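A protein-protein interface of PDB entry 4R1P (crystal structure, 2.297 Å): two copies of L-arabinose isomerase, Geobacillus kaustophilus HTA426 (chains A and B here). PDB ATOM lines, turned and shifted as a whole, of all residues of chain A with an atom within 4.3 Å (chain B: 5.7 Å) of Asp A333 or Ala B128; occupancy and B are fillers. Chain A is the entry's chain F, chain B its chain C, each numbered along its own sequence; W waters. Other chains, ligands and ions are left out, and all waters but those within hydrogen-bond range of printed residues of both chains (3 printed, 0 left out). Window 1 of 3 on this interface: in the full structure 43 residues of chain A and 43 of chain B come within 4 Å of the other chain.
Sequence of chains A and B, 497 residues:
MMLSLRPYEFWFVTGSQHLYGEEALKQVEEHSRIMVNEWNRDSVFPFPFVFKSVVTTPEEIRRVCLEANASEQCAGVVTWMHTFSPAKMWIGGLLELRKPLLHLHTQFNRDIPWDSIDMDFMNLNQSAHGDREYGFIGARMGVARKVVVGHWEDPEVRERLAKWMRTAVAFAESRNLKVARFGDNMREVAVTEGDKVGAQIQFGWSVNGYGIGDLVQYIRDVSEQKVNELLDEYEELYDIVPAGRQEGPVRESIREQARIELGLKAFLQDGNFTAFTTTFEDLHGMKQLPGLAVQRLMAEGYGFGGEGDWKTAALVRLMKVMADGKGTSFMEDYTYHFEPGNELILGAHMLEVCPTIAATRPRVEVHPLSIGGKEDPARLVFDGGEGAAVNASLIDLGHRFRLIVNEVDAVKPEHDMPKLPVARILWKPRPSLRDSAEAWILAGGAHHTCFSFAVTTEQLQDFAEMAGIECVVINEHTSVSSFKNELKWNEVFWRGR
A ring nitrogen (ND1) of His B105 is in hydrogen-bond range of the side-chain carboxylate (OD2) of Asp B131. The side-chain amide oxygen (OE1) of Gln B126 lies within hydrogen-bond range of a ring nitrogen (NE2) of His B129, 3.0 Å away. N of Tyr A334 sits at hydrogen-bond distance from O of Leu A346 (2.9 Å). N of Leu A346 lies within hydrogen-bond range of O of Thr A335 (2.8 Å).
Hydrophobic or aromatic side chains of chain B that line the printed part of chain A: His B105, Ala B128 and His B129. Printed residues of chain A that touch a printed residue of chain B: Glu A332, Asp A333, Tyr A334, Thr A335, Tyr A336 and His A447. Among the printed residues, Asp or Glu carboxylates within 4 Å of a Lys or Arg side-chain nitrogen of the other chain: Asp A333 with Arg B132.
A ring nitrogen (NE2) of His B105 is in hydrogen-bond range of the side-chain hydroxyl (OH) of Tyr A336 (2.8 Å). OE1 of Gln B107 is in hydrogen-bond range of OG1 of Thr A335 (3.1 Å). N of Tyr A336 sits at hydrogen-bond distance from OE1 of Gln B107. O of Asn B125 is in hydrogen-bond range of OG1 of Thr A335, 3.3 Å away. OE2 of Glu A332 lies close to NE2 of His B129 (3.4 Å). A ring nitrogen (ND1) of His B129 lies within hydrogen-bond range of the backbone carbonyl oxygen (O) of Asp A333 (2.8 Å). The guanidinium group (NH1) of Arg B132 lies within salt-bridge range of the side-chain carboxylate (OD1) of Asp A333, at 3.1 Å. The guanidinium group (NH1) of Arg B132 is in hydrogen-bond range of the side-chain hydroxyl (OH) of Tyr A336 (2.7 Å).
No position is printed for both chains. Of the 16 pairs that touch across the chains among the printed residues, none has its exchanged pair printed and touching as well.
Among the printed residues, pairs that only touch across the chains: Asp A333 with Ala B128 (3.7 Å), Tyr A334 with Asn B125 (3.6 Å), Tyr A334 with Gln B126 (3.5 Å), Tyr A334 with Ala B128 (3.5 Å), Tyr A334 with His B129 (3.6 Å), Thr A335 with Ala B128 (3.4 Å), Tyr A336 with Ala B128 (3.8 Å) and His A447 with His B129 (3.4 Å).
Water W1 lies within hydrogen-bond range of OG1 of Thr A335 (2.5 Å), O of Tyr A336 (2.9 Å) and NE2 of Gln B107 (3.5 Å). Water W2 lies within hydrogen-bond range of OD2 of Asp A333 (2.7 Å) and NE of Arg B132 (2.8 Å). Water W3 bridges OH of Tyr A334 (2.8 Å) and OE1 of Gln B126 (3.3 Å).
Of the printed residues of chain A, Asn B125 touches Tyr A334 and Thr A335. Of the printed residues of chain A, Gln B126 touches Tyr A334. Ser B127 touches none of the printed residues of chain A. Gly B130 touches none of the printed residues of chain A. The nearest residue of chain B that does not touch Asp A333 is Gln B126 (5.4 Å). The nearest printed residue of chain B that does not touch Thr A335 is Gln B126 (5.5 Å).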
ATOM      1  N   GLU A 332      23.083 -17.483  -8.091  1.00  0.00           N
ATOM      2  CA  GLU A 332      23.828 -18.376  -7.218  1.00  0.00           C
ATOM      3  C   GLU A 332      22.830 -19.191  -6.392  1.00  0.00           C
ATOM      4  O   GLU A 332      21.896 -18.624  -5.836  1.00  0.00           O
ATOM      5  CB  GLU A 332      24.739 -17.561  -6.292  1.00  0.00           C
ATOM      6  CG  GLU A 332      25.619 -18.399  -5.362  1.00  0.00           C
ATOM      7  CD  GLU A 332      26.721 -17.582  -4.682  1.00  0.00           C
ATOM      8  OE1 GLU A 332      26.685 -16.344  -4.745  1.00  0.00           O
ATOM      9  OE2 GLU A 332      27.634 -18.178  -4.069  1.00  0.00           O
ATOM     10  N   ASP A 333      23.014 -20.509  -6.324  1.00  0.00           N
ATOM     11  CA  ASP A 333      22.215 -21.353  -5.425  1.00  0.00           C
ATOM     12  C   ASP A 333      22.552 -20.978  -3.996  1.00  0.00           C
ATOM     13  O   ASP A 333      23.693 -21.149  -3.569  1.00  0.00           O
ATOM     14  CB  ASP A 333      22.536 -22.850  -5.595  1.00  0.00           C
ATOM     15  CG  ASP A 333      22.561 -23.297  -7.044  1.00  0.00           C
ATOM     16  OD1 ASP A 333      21.893 -24.311  -7.365  1.00  0.00           O
ATOM     17  OD2 ASP A 333      23.267 -22.656  -7.858  1.00  0.00           O
ATOM     18  N   TYR A 334      21.575 -20.488  -3.241  1.00  0.00           N
ATOM     19  CA  TYR A 334      21.860 -20.068  -1.872  1.00  0.00           C
ATOM     20  C   TYR A 334      21.484 -21.058  -0.779  1.00  0.00           C
ATOM     21  O   TYR A 334      22.237 -21.219   0.190  1.00  0.00           O
ATOM     22  CB  TYR A 334      21.250 -18.701  -1.576  1.00  0.00           C
ATOM     23  CG  TYR A 334      22.297 -17.655  -1.296  1.00  0.00           C
ATOM     24  CD1 TYR A 334      22.790 -16.850  -2.318  1.00  0.00           C
ATOM     25  CD2 TYR A 334      22.819 -17.488  -0.011  1.00  0.00           C
ATOM     26  CE1 TYR A 334      23.754 -15.892  -2.067  1.00  0.00           C
ATOM     27  CE2 TYR A 334      23.785 -16.526   0.252  1.00  0.00           C
ATOM     28  CZ  TYR A 334      24.250 -15.734  -0.782  1.00  0.00           C
ATOM     29  OH  TYR A 334      25.213 -14.778  -0.548  1.00  0.00           O
ATOM     30  N   THR A 335      20.330 -21.708  -0.915  1.00  0.00           N
ATOM     31  CA  THR A 335      19.854 -22.616   0.136  1.00  0.00           C
ATOM     32  C   THR A 335      18.759 -23.585  -0.324  1.00  0.00           C
ATOM     33  O   THR A 335      18.057 -23.343  -1.314  1.00  0.00           O
ATOM     34  CB  THR A 335      19.428 -21.841   1.422  1.00  0.00           C
ATOM     35  OG1 THR A 335      19.343 -22.743   2.538  1.00  0.00           O
ATOM     36  CG2 THR A 335      18.091 -21.130   1.219  1.00  0.00           C
ATOM     37  N   TYR A 336      18.631 -24.696   0.393  1.00  0.00           N
ATOM     38  CA  TYR A 336      17.738 -25.766  -0.021  1.00  0.00           C
ATOM     39  C   TYR A 336      16.496 -25.893   0.865  1.00  0.00           C
ATOM     40  O   TYR A 336      16.523 -25.578   2.053  1.00  0.00           O
ATOM     41  CB  TYR A 336      18.478 -27.107  -0.039  1.00  0.00           C
ATOM     42  CG  TYR A 336      19.464 -27.321  -1.171  1.00  0.00           C
ATOM     43  CD1 TYR A 336      19.405 -26.583  -2.344  1.00  0.00           C
ATOM     44  CD2 TYR A 336      20.456 -28.279  -1.063  1.00  0.00           C
ATOM     45  CE1 TYR A 336      20.321 -26.799  -3.378  1.00  0.00           C
ATOM     46  CE2 TYR A 336      21.364 -28.495  -2.080  1.00  0.00           C
ATOM     47  CZ  TYR A 336      21.299 -27.755  -3.234  1.00  0.00           C
ATOM     48  OH  TYR A 336      22.223 -27.993  -4.228  1.00  0.00           O
ATOM     49  N   ILE A 345      15.207 -25.154  -4.668  1.00  0.00           N
ATOM     50  CA  ILE A 345      16.401 -24.370  -4.414  1.00  0.00           C
ATOM     51  C   ILE A 345      16.021 -22.905  -4.389  1.00  0.00           C
ATOM     52  O   ILE A 345      15.248 -22.449  -5.236  1.00  0.00           O
ATOM     53  CB  ILE A 345      17.438 -24.562  -5.527  1.00  0.00           C
ATOM     54  CG1 ILE A 345      17.654 -26.051  -5.811  1.00  0.00           C
ATOM     55  CG2 ILE A 345      18.754 -23.827  -5.189  1.00  0.00           C
ATOM     56  CD1 ILE A 345      18.696 -26.318  -6.893  1.00  0.00           C
ATOM     57  N   LEU A 346      16.555 -22.166  -3.419  1.00  0.00           N
ATOM     58  CA  LEU A 346      16.370 -20.722  -3.389  1.00  0.00           C
ATOM     59  C   LEU A 346      17.653 -20.081  -3.902  1.00  0.00           C
ATOM     60  O   LEU A 346      18.730 -20.319  -3.347  1.00  0.00           O
ATOM     61  CB  LEU A 346      16.056 -20.257  -1.962  1.00  0.00           C
ATOM     62  CG  LEU A 346      15.758 -18.774  -1.723  1.00  0.00           C
ATOM     63  CD1 LEU A 346      14.860 -18.605  -0.526  1.00  0.00           C
ATOM     64  CD2 LEU A 346      17.035 -17.971  -1.511  1.00  0.00           C
ATOM     65  N   TRP A 427      13.386 -22.502  -7.589  1.00  0.00           N
ATOM     66  CA  TRP A 427      13.209 -23.451  -8.694  1.00  0.00           C
ATOM     67  C   TRP A 427      13.322 -24.922  -8.310  1.00  0.00           C
ATOM     68  O   TRP A 427      14.041 -25.287  -7.383  1.00  0.00           O
ATOM     69  CB  TRP A 427      14.136 -23.128  -9.880  1.00  0.00           C
ATOM     70  CG  TRP A 427      15.601 -23.401  -9.637  1.00  0.00           C
ATOM     71  CD1 TRP A 427      16.250 -24.602  -9.764  1.00  0.00           C
ATOM     72  CD2 TRP A 427      16.597 -22.448  -9.258  1.00  0.00           C
ATOM     73  NE1 TRP A 427      17.587 -24.452  -9.471  1.00  0.00           N
ATOM     74  CE2 TRP A 427      17.825 -23.138  -9.164  1.00  0.00           C
ATOM     75  CE3 TRP A 427      16.570 -21.075  -8.988  1.00  0.00           C
ATOM     76  CZ2 TRP A 427      19.006 -22.504  -8.803  1.00  0.00           C
ATOM     77  CZ3 TRP A 427      17.750 -20.446  -8.636  1.00  0.00           C
ATOM     78  CH2 TRP A 427      18.951 -21.157  -8.547  1.00  0.00           C
ATOM     79  N   HIS A 447      29.012 -22.626  -8.579  1.00  0.00           N
ATOM     80  CA  HIS A 447      27.982 -22.084  -7.713  1.00  0.00           C
ATOM     81  C   HIS A 447      27.359 -20.837  -8.337  1.00  0.00           C
ATOM     82  O   HIS A 447      26.223 -20.480  -8.021  1.00  0.00           O
ATOM     83  CB  HIS A 447      28.566 -21.774  -6.338  1.00  0.00           C
ATOM     84  CG  HIS A 447      29.598 -20.690  -6.344  1.00  0.00           C
ATOM     85  ND1 HIS A 447      30.752 -20.760  -7.095  1.00  0.00           N
ATOM     86  CD2 HIS A 447      29.659 -19.513  -5.676  1.00  0.00           C
ATOM     87  CE1 HIS A 447      31.471 -19.667  -6.903  1.00  0.00           C
ATOM     88  NE2 HIS A 447      30.827 -18.890  -6.049  1.00  0.00           N
ATOM     89  N   HIS B 105      26.583 -33.846   0.367  1.00  0.00           N
ATOM     90  CA  HIS B 105      25.920 -32.614   0.031  1.00  0.00           C
ATOM     91  C   HIS B 105      24.624 -32.541   0.842  1.00  0.00           C
ATOM     92  O   HIS B 105      23.581 -33.059   0.429  1.00  0.00           O
ATOM     93  CB  HIS B 105      25.632 -32.599  -1.469  1.00  0.00           C
ATOM     94  CG  HIS B 105      25.117 -31.292  -1.975  1.00  0.00           C
ATOM     95  ND1 HIS B 105      25.362 -30.099  -1.334  1.00  0.00           N
ATOM     96  CD2 HIS B 105      24.377 -30.988  -3.065  1.00  0.00           C
ATOM     97  CE1 HIS B 105      24.796 -29.113  -2.009  1.00  0.00           C
ATOM     98  NE2 HIS B 105      24.187 -29.627  -3.061  1.00  0.00           N
ATOM     99  N   THR B 106      24.703 -31.906   2.007  1.00  0.00           N
ATOM    100  CA  THR B 106      23.581 -31.870   2.938  1.00  0.00           C
ATOM    101  C   THR B 106      23.337 -30.458   3.505  1.00  0.00           C
ATOM    102  O   THR B 106      23.893 -29.472   3.025  1.00  0.00           O
ATOM    103  CB  THR B 106      23.790 -32.912   4.071  1.00  0.00           C
ATOM    104  OG1 THR B 106      22.571 -33.109   4.799  1.00  0.00           O
ATOM    105  CG2 THR B 106      24.885 -32.475   5.011  1.00  0.00           C
ATOM    106  N   GLN B 107      22.484 -30.366   4.515  1.00  0.00           N
ATOM    107  CA  GLN B 107      22.075 -29.089   5.077  1.00  0.00           C
ATOM    108  C   GLN B 107      21.597 -29.432   6.474  1.00  0.00           C
ATOM    109  O   GLN B 107      21.025 -30.510   6.659  1.00  0.00           O
ATOM    110  CB  GLN B 107      20.929 -28.520   4.245  1.00  0.00           C
ATOM    111  CG  GLN B 107      20.598 -27.075   4.506  1.00  0.00           C
ATOM    112  CD  GLN B 107      19.547 -26.547   3.546  1.00  0.00           C
ATOM    113  OE1 GLN B 107      19.861 -25.818   2.605  1.00  0.00           O
ATOM    114  NE2 GLN B 107      18.291 -26.909   3.780  1.00  0.00           N
ATOM    115  N   ASN B 125      23.920 -21.176   6.231  1.00  0.00           N
ATOM    116  CA  ASN B 125      23.452 -22.451   5.721  1.00  0.00           C
ATOM    117  C   ASN B 125      23.481 -22.449   4.201  1.00  0.00           C
ATOM    118  O   ASN B 125      22.439 -22.512   3.540  1.00  0.00           O
ATOM    119  CB  ASN B 125      22.037 -22.736   6.238  1.00  0.00           C
ATOM    120  CG  ASN B 125      21.952 -22.685   7.762  1.00  0.00           C
ATOM    121  OD1 ASN B 125      22.402 -23.602   8.455  1.00  0.00           O
ATOM    122  ND2 ASN B 125      21.367 -21.610   8.287  1.00  0.00           N
ATOM    123  N   GLN B 126      24.689 -22.377   3.657  1.00  0.00           N
ATOM    124  CA  GLN B 126      24.870 -22.178   2.227  1.00  0.00           C
ATOM    125  C   GLN B 126      25.659 -23.310   1.566  1.00  0.00           C
ATOM    126  O   GLN B 126      26.467 -23.079   0.656  1.00  0.00           O
ATOM    127  CB  GLN B 126      25.541 -20.828   1.973  1.00  0.00           C
ATOM    128  CG  GLN B 126      26.862 -20.617   2.696  1.00  0.00           C
ATOM    129  CD  GLN B 126      27.467 -19.249   2.392  1.00  0.00           C
ATOM    130  OE1 GLN B 126      26.757 -18.314   2.003  1.00  0.00           O
ATOM    131  NE2 GLN B 126      28.779 -19.129   2.551  1.00  0.00           N
ATOM    132  N   SER B 127      25.410 -24.533   2.031  1.00  0.00           N
ATOM    133  CA  SER B 127      25.954 -25.726   1.398  1.00  0.00           C
ATOM    134  C   SER B 127      25.524 -25.747  -0.055  1.00  0.00           C
ATOM    135  O   SER B 127      26.238 -26.269  -0.915  1.00  0.00           O
ATOM    136  CB  SER B 127      25.446 -26.989   2.095  1.00  0.00           C
ATOM    137  OG  SER B 127      26.040 -27.159   3.368  1.00  0.00           O
ATOM    138  N   ALA B 128      24.350 -25.171  -0.316  1.00  0.00           N
ATOM    139  CA  ALA B 128      23.820 -25.066  -1.667  1.00  0.00           C
ATOM    140  C   ALA B 128      24.872 -24.517  -2.619  1.00  0.00           C
ATOM    141  O   ALA B 128      24.921 -24.923  -3.766  1.00  0.00           O
ATOM    142  CB  ALA B 128      22.578 -24.198  -1.700  1.00  0.00           C
ATOM    143  N   HIS B 129      25.715 -23.598  -2.151  1.00  0.00           N
ATOM    144  CA  HIS B 129      26.823 -23.180  -2.993  1.00  0.00           C
ATOM    145  C   HIS B 129      28.219 -23.612  -2.537  1.00  0.00           C
ATOM    146  O   HIS B 129      29.106 -23.798  -3.369  1.00  0.00           O
ATOM    147  CB  HIS B 129      26.746 -21.702  -3.431  1.00  0.00           C
ATOM    148  CG  HIS B 129      26.727 -20.696  -2.320  1.00  0.00           C
ATOM    149  ND1 HIS B 129      25.556 -20.223  -1.763  1.00  0.00           N
ATOM    150  CD2 HIS B 129      27.730 -20.000  -1.727  1.00  0.00           C
ATOM    151  CE1 HIS B 129      25.841 -19.308  -0.853  1.00  0.00           C
ATOM    152  NE2 HIS B 129      27.152 -19.154  -0.810  1.00  0.00           N
ATOM    153  N   GLY B 130      28.404 -23.804  -1.235  1.00  0.00           N
ATOM    154  CA  GLY B 130      29.683 -24.255  -0.722  1.00  0.00           C
ATOM    155  C   GLY B 130      30.114 -25.605  -1.275  1.00  0.00           C
ATOM    156  O   GLY B 130      31.302 -25.812  -1.527  1.00  0.00           O
ATOM    157  N   ASP B 131      29.153 -26.511  -1.472  1.00  0.00           N
ATOM    158  CA  ASP B 131      29.433 -27.875  -1.935  1.00  0.00           C
ATOM    159  C   ASP B 131      29.691 -27.939  -3.438  1.00  0.00           C
ATOM    160  O   ASP B 131      30.325 -28.873  -3.935  1.00  0.00           O
ATOM    161  CB  ASP B 131      28.272 -28.815  -1.605  1.00  0.00           C
ATOM    162  CG  ASP B 131      28.269 -29.263  -0.148  1.00  0.00           C
ATOM    163  OD1 ASP B 131      29.343 -29.614   0.393  1.00  0.00           O
ATOM    164  OD2 ASP B 131      27.176 -29.262   0.463  1.00  0.00           O
ATOM    165  N   ARG B 132      29.173 -26.961  -4.166  1.00  0.00           N
ATOM    166  CA  ARG B 132      29.394 -26.898  -5.603  1.00  0.00           C
ATOM    167  C   ARG B 132      30.799 -26.363  -5.936  1.00  0.00           C
ATOM    168  O   ARG B 132      31.470 -26.883  -6.828  1.00  0.00           O
ATOM    169  CB  ARG B 132      28.292 -26.079  -6.266  1.00  0.00           C
ATOM    170  CG  ARG B 132      26.909 -26.739  -6.111  1.00  0.00           C
ATOM    171  CD  ARG B 132      25.790 -25.763  -6.381  1.00  0.00           C
ATOM    172  NE  ARG B 132      25.056 -26.063  -7.594  1.00  0.00           N
ATOM    173  CZ  ARG B 132      23.857 -26.636  -7.637  1.00  0.00           C
ATOM    174  NH1 ARG B 132      23.229 -26.982  -6.523  1.00  0.00           N
ATOM    175  NH2 ARG B 132      23.291 -26.870  -8.811  1.00  0.00           N
HETATM  176  O   HOH W   1      17.411 -23.553   3.991  1.00  0.00           O
HETATM  177  O   HOH W   2      24.760 -24.128  -9.590  1.00  0.00           O
HETATM  178  O   HOH W   3      26.595 -15.007   1.894  1.00  0.00           O
